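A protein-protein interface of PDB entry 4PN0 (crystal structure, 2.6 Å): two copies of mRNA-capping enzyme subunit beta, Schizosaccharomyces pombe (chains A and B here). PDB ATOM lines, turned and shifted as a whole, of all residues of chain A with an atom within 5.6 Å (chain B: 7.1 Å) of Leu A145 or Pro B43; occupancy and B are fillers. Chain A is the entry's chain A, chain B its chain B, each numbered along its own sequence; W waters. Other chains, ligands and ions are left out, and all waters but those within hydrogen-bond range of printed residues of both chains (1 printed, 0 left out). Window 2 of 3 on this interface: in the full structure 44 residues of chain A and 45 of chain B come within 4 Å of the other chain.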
ATOM      1  N   SER A 139     -16.662 -30.670  31.435  1.00  0.00           N
ATOM      2  CA  SER A 139     -17.697 -29.666  31.214  1.00  0.00           C
ATOM      3  C   SER A 139     -17.540 -28.468  32.145  1.00  0.00           C
ATOM      4  O   SER A 139     -18.196 -27.442  31.966  1.00  0.00           O
ATOM      5  CB  SER A 139     -19.083 -30.277  31.413  1.00  0.00           C
ATOM      6  OG  SER A 139     -19.340 -30.490  32.789  1.00  0.00           O
ATOM      7  N   GLY A 143     -15.532 -22.150  29.036  1.00  0.00           N
ATOM      8  CA  GLY A 143     -15.991 -22.202  27.661  1.00  0.00           C
ATOM      9  C   GLY A 143     -17.030 -23.279  27.415  1.00  0.00           C
ATOM     10  O   GLY A 143     -17.708 -23.277  26.387  1.00  0.00           O
ATOM     11  N   ARG A 144     -17.159 -24.203  28.362  1.00  0.00           N
ATOM     12  CA  ARG A 144     -18.099 -25.310  28.229  1.00  0.00           C
ATOM     13  C   ARG A 144     -19.409 -25.057  28.968  1.00  0.00           C
ATOM     14  O   ARG A 144     -19.498 -24.165  29.813  1.00  0.00           O
ATOM     15  CB  ARG A 144     -17.467 -26.603  28.747  1.00  0.00           C
ATOM     16  CG  ARG A 144     -16.396 -27.179  27.844  1.00  0.00           C
ATOM     17  CD  ARG A 144     -17.004 -27.759  26.580  1.00  0.00           C
ATOM     18  NE  ARG A 144     -18.093 -28.685  26.877  1.00  0.00           N
ATOM     19  CZ  ARG A 144     -17.918 -29.942  27.273  1.00  0.00           C
ATOM     20  NH1 ARG A 144     -16.693 -30.428  27.430  1.00  0.00           N
ATOM     21  NH2 ARG A 144     -18.969 -30.711  27.516  1.00  0.00           N
ATOM     22  N   LEU A 145     -20.426 -25.845  28.632  1.00  0.00           N
ATOM     23  CA  LEU A 145     -21.671 -25.850  29.387  1.00  0.00           C
ATOM     24  C   LEU A 145     -21.589 -26.934  30.454  1.00  0.00           C
ATOM     25  O   LEU A 145     -21.468 -28.118  30.134  1.00  0.00           O
ATOM     26  CB  LEU A 145     -22.871 -26.091  28.474  1.00  0.00           C
ATOM     27  CG  LEU A 145     -23.129 -25.022  27.411  1.00  0.00           C
ATOM     28  CD1 LEU A 145     -24.449 -25.286  26.702  1.00  0.00           C
ATOM     29  CD2 LEU A 145     -23.110 -23.630  28.026  1.00  0.00           C
ATOM     30  N   PRO A 146     -21.653 -26.524  31.728  1.00  0.00           N
ATOM     31  CA  PRO A 146     -21.415 -27.385  32.891  1.00  0.00           C
ATOM     32  C   PRO A 146     -22.409 -28.532  33.035  1.00  0.00           C
ATOM     33  O   PRO A 146     -23.591 -28.378  32.731  1.00  0.00           O
ATOM     34  CB  PRO A 146     -21.576 -26.427  34.077  1.00  0.00           C
ATOM     35  CG  PRO A 146     -21.397 -25.061  33.505  1.00  0.00           C
ATOM     36  CD  PRO A 146     -21.961 -25.141  32.124  1.00  0.00           C
ATOM     37  N   PHE A 147     -21.907 -29.673  33.498  1.00  0.00           N
ATOM     38  CA  PHE A 147     -22.738 -30.790  33.922  1.00  0.00           C
ATOM     39  C   PHE A 147     -23.275 -30.505  35.316  1.00  0.00           C
ATOM     40  O   PHE A 147     -22.627 -29.821  36.110  1.00  0.00           O
ATOM     41  CB  PHE A 147     -21.896 -32.059  34.002  1.00  0.00           C
ATOM     42  CG  PHE A 147     -22.130 -33.024  32.882  1.00  0.00           C
ATOM     43  CD1 PHE A 147     -23.223 -33.873  32.899  1.00  0.00           C
ATOM     44  CD2 PHE A 147     -21.237 -33.107  31.826  1.00  0.00           C
ATOM     45  CE1 PHE A 147     -23.432 -34.776  31.871  1.00  0.00           C
ATOM     46  CE2 PHE A 147     -21.439 -34.007  30.796  1.00  0.00           C
ATOM     47  CZ  PHE A 147     -22.538 -34.843  30.819  1.00  0.00           C
ATOM     48  N   HIS A 235     -27.154 -32.285  31.609  1.00  0.00           N
ATOM     49  CA  HIS A 235     -26.493 -31.382  30.679  1.00  0.00           C
ATOM     50  C   HIS A 235     -27.502 -30.873  29.662  1.00  0.00           C
ATOM     51  O   HIS A 235     -28.155 -31.665  28.983  1.00  0.00           O
ATOM     52  CB  HIS A 235     -25.341 -32.093  29.971  1.00  0.00           C
ATOM     53  CG  HIS A 235     -24.488 -31.185  29.142  1.00  0.00           C
ATOM     54  ND1 HIS A 235     -24.666 -31.031  27.783  1.00  0.00           N
ATOM     55  CD2 HIS A 235     -23.450 -30.384  29.478  1.00  0.00           C
ATOM     56  CE1 HIS A 235     -23.773 -30.175  27.320  1.00  0.00           C
ATOM     57  NE2 HIS A 235     -23.022 -29.768  28.328  1.00  0.00           N
ATOM     58  N   GLN A 236     -27.625 -29.552  29.570  1.00  0.00           N
ATOM     59  CA  GLN A 236     -28.587 -28.913  28.672  1.00  0.00           C
ATOM     60  C   GLN A 236     -29.992 -29.472  28.864  1.00  0.00           C
ATOM     61  O   GLN A 236     -30.699 -29.745  27.892  1.00  0.00           O
ATOM     62  CB  GLN A 236     -28.148 -29.049  27.213  1.00  0.00           C
ATOM     63  CG  GLN A 236     -26.891 -28.267  26.880  1.00  0.00           C
ATOM     64  CD  GLN A 236     -26.517 -28.358  25.416  1.00  0.00           C
ATOM     65  OE1 GLN A 236     -26.260 -27.344  24.765  1.00  0.00           O
ATOM     66  NE2 GLN A 236     -26.476 -29.577  24.888  1.00  0.00           N
ATOM     67  N   ALA B  41     -17.366 -16.233  27.680  1.00  0.00           N
ATOM     68  CA  ALA B  41     -17.074 -16.998  26.473  1.00  0.00           C
ATOM     69  C   ALA B  41     -17.761 -18.360  26.492  1.00  0.00           C
ATOM     70  O   ALA B  41     -17.141 -19.382  26.196  1.00  0.00           O
ATOM     71  CB  ALA B  41     -15.569 -17.162  26.296  1.00  0.00           C
ATOM     72  N   VAL B  42     -19.044 -18.370  26.845  1.00  0.00           N
ATOM     73  CA  VAL B  42     -19.832 -19.599  26.844  1.00  0.00           C
ATOM     74  C   VAL B  42     -20.851 -19.588  25.704  1.00  0.00           C
ATOM     75  O   VAL B  42     -21.379 -18.533  25.345  1.00  0.00           O
ATOM     76  CB  VAL B  42     -20.541 -19.833  28.203  1.00  0.00           C
ATOM     77  CG1 VAL B  42     -19.526 -19.831  29.337  1.00  0.00           C
ATOM     78  CG2 VAL B  42     -21.620 -18.786  28.446  1.00  0.00           C
ATOM     79  N   PRO B  43     -21.117 -20.765  25.115  1.00  0.00           N
ATOM     80  CA  PRO B  43     -22.040 -20.853  23.980  1.00  0.00           C
ATOM     81  C   PRO B  43     -23.493 -20.950  24.427  1.00  0.00           C
ATOM     82  O   PRO B  43     -23.767 -21.140  25.613  1.00  0.00           O
ATOM     83  CB  PRO B  43     -21.619 -22.157  23.303  1.00  0.00           C
ATOM     84  CG  PRO B  43     -21.144 -23.006  24.428  1.00  0.00           C
ATOM     85  CD  PRO B  43     -20.499 -22.068  25.423  1.00  0.00           C
ATOM     86  N   LYS B  44     -24.414 -20.817  23.481  1.00  0.00           N
ATOM     87  CA  LYS B  44     -25.828 -20.966  23.783  1.00  0.00           C
ATOM     88  C   LYS B  44     -26.202 -22.441  23.796  1.00  0.00           C
ATOM     89  O   LYS B  44     -26.835 -22.922  24.736  1.00  0.00           O
ATOM     90  CB  LYS B  44     -26.682 -20.201  22.770  1.00  0.00           C
ATOM     91  CG  LYS B  44     -26.410 -18.708  22.750  1.00  0.00           C
ATOM     92  CD  LYS B  44     -27.432 -17.962  21.914  1.00  0.00           C
ATOM     93  CE  LYS B  44     -27.184 -16.463  21.969  1.00  0.00           C
ATOM     94  NZ  LYS B  44     -28.243 -15.695  21.258  1.00  0.00           N
ATOM     95  N   ILE B  45     -25.800 -23.155  22.749  1.00  0.00           N
ATOM     96  CA  ILE B  45     -26.109 -24.575  22.622  1.00  0.00           C
ATOM     97  C   ILE B  45     -24.857 -25.389  22.298  1.00  0.00           C
ATOM     98  O   ILE B  45     -23.998 -24.947  21.536  1.00  0.00           O
ATOM     99  CB  ILE B  45     -27.166 -24.828  21.517  1.00  0.00           C
ATOM    100  CG1 ILE B  45     -28.350 -23.868  21.660  1.00  0.00           C
ATOM    101  CG2 ILE B  45     -27.649 -26.273  21.549  1.00  0.00           C
ATOM    102  CD1 ILE B  45     -29.207 -24.124  22.880  1.00  0.00           C
ATOM    103  N   GLU B  46     -24.753 -26.572  22.893  1.00  0.00           N
ATOM    104  CA  GLU B  46     -23.744 -27.546  22.497  1.00  0.00           C
ATOM    105  C   GLU B  46     -24.442 -28.707  21.800  1.00  0.00           C
ATOM    106  O   GLU B  46     -25.594 -29.015  22.104  1.00  0.00           O
ATOM    107  CB  GLU B  46     -22.954 -28.039  23.710  1.00  0.00           C
ATOM    108  CG  GLU B  46     -22.061 -26.978  24.337  1.00  0.00           C
ATOM    109  CD  GLU B  46     -21.181 -27.528  25.445  1.00  0.00           C
ATOM    110  OE1 GLU B  46     -20.295 -26.789  25.926  1.00  0.00           O
ATOM    111  OE2 GLU B  46     -21.372 -28.698  25.835  1.00  0.00           O
ATOM    112  N   ASN B  48     -23.693 -31.856  21.891  1.00  0.00           N
ATOM    113  CA  ASN B  48     -23.748 -33.013  22.780  1.00  0.00           C
ATOM    114  C   ASN B  48     -23.001 -32.689  24.065  1.00  0.00           C
ATOM    115  O   ASN B  48     -22.417 -31.613  24.184  1.00  0.00           O
ATOM    116  CB  ASN B  48     -23.145 -34.248  22.116  1.00  0.00           C
ATOM    117  CG  ASN B  48     -21.842 -33.950  21.417  1.00  0.00           C
ATOM    118  OD1 ASN B  48     -20.821 -33.711  22.061  1.00  0.00           O
ATOM    119  ND2 ASN B  48     -21.870 -33.959  20.090  1.00  0.00           N
ATOM    120  N   PHE B  49     -23.007 -33.607  25.026  1.00  0.00           N
ATOM    121  CA  PHE B  49     -22.347 -33.329  26.300  1.00  0.00           C
ATOM    122  C   PHE B  49     -20.821 -33.415  26.219  1.00  0.00           C
ATOM    123  O   PHE B  49     -20.126 -33.206  27.214  1.00  0.00           O
ATOM    124  CB  PHE B  49     -22.908 -34.199  27.438  1.00  0.00           C
ATOM    125  CG  PHE B  49     -22.681 -35.679  27.261  1.00  0.00           C
ATOM    126  CD1 PHE B  49     -21.446 -36.247  27.528  1.00  0.00           C
ATOM    127  CD2 PHE B  49     -23.718 -36.505  26.867  1.00  0.00           C
ATOM    128  CE1 PHE B  49     -21.243 -37.605  27.375  1.00  0.00           C
ATOM    129  CE2 PHE B  49     -23.522 -37.863  26.715  1.00  0.00           C
ATOM    130  CZ  PHE B  49     -22.282 -38.414  26.970  1.00  0.00           C
ATOM    131  N   ASN B  51     -19.383 -31.777  23.523  1.00  0.00           N
ATOM    132  CA  ASN B  51     -19.112 -30.622  22.670  1.00  0.00           C
ATOM    133  C   ASN B  51     -18.235 -31.038  21.492  1.00  0.00           C
ATOM    134  O   ASN B  51     -17.293 -30.341  21.115  1.00  0.00           O
ATOM    135  CB  ASN B  51     -18.463 -29.492  23.474  1.00  0.00           C
ATOM    136  CG  ASN B  51     -18.438 -28.180  22.721  1.00  0.00           C
ATOM    137  OD1 ASN B  51     -19.385 -27.839  22.011  1.00  0.00           O
ATOM    138  ND2 ASN B  51     -17.345 -27.438  22.865  1.00  0.00           N
HETATM  139  O   HOH W   1     -15.447 -29.542  24.383  1.00  0.00           O
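Leu A145 touches just these residues of chain B: Pro B43 (3.5 Å), Lys B44 (3.9 Å) and Glu B46 (2.9 Å). Of the printed residues of chain B, Gly A143 touches Ala B41 (3.4 Å) and Pro B43 (3.2 Å). Of the printed residues of chain B, Phe A147 touches Phe B49 (3.5 Å). Of the printed residues of chain B, Arg A144 touches Glu B46, Phe B49 and Asn B51. Of the printed residues of chain A, Ala B41 touches Gly A143. Ser A139 touches none of the printed residues of chain B. Pro A146 touches none of the printed residues of chain B. The nearest residue of chain B that does not touch Leu A145 is Ile B45 (4.4 Å).
Water W1 lies within hydrogen-bond range of ND2 of Asn B51 (3.2 Å) and NH1 of Arg A144 (3.4 Å).
NH2 of Arg A144 lies within hydrogen-bond range of O of Phe B49, at 2.8 Å. N of Leu A145 lies within hydrogen-bond range of OE1 of Glu B46, 2.9 Å away. A ring nitrogen (NE2) of His A235 sits at hydrogen-bond distance from the side-chain carboxylate of Glu B46 (3.2 Å). The side-chain amide oxygen (OE1) of Gln A236 is in hydrogen-bond range of the backbone NH (N) of Glu B46. The guanidinium group of Arg A144 is in salt-bridge range of the side-chain carboxylate of Glu B46.
OG of Ser A139 sits at hydrogen-bond distance from N of Phe A147 (2.8 Å). OD1 of Asn B48 is in hydrogen-bond range of N of Asn B51 (2.8 Å). The backbone carbonyl oxygen (O) of Leu A145 is in hydrogen-bond range of a ring nitrogen (NE2) of His A235, at 2.9 Å.
No position is printed for both chains. Of the 14 pairs that touch across the chains among the printed residues, none has its exchanged pair printed and touching as well.
CA of Gly A143 touches O of Ala B41, at 3.4 Å. CD of Pro B43 touches O of Gly A143, 3.2 Å away. CB of Asn B51 touches NE of Arg A144 (3.5 Å). Leu A145 touches Pro B43. Lys B44 touches Leu A145 (O to CD1, 3.9 Å). Phe A147 touches Phe B49. His A235 touches Asn B48. ND1 of His A235 touches CA of Phe B49, 3.6 Å away. OE1 of Gln A236 touches C of Ile B45, 3.4 Å away.
Of the 9 printed residues of chain B, 8 touch a printed residue of chain A. Hydrophobic or aromatic side chains of chain B that line the printed part of chain A: Pro B43, Ile B45 and Phe B49. Of the 8 printed residues of chain A, 6 touch a printed residue of chain B. Printed residues of chain A that touch a printed residue of chain B: Gly A143, Arg A144, Leu A145, Phe A147, His A235 and Gln A236. Hydrophobic or aromatic side chains of chain A that line the printed part of chain B: Leu A145, Phe A147 and His A235. Among the printed residues, 14 pairs touch across the chains. Among the printed residues, Asp or Glu carboxylates within 4 Å of a Lys or Arg side-chain nitrogen of the other chain: Arg A144 with Glu B46 (3.1 Å).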
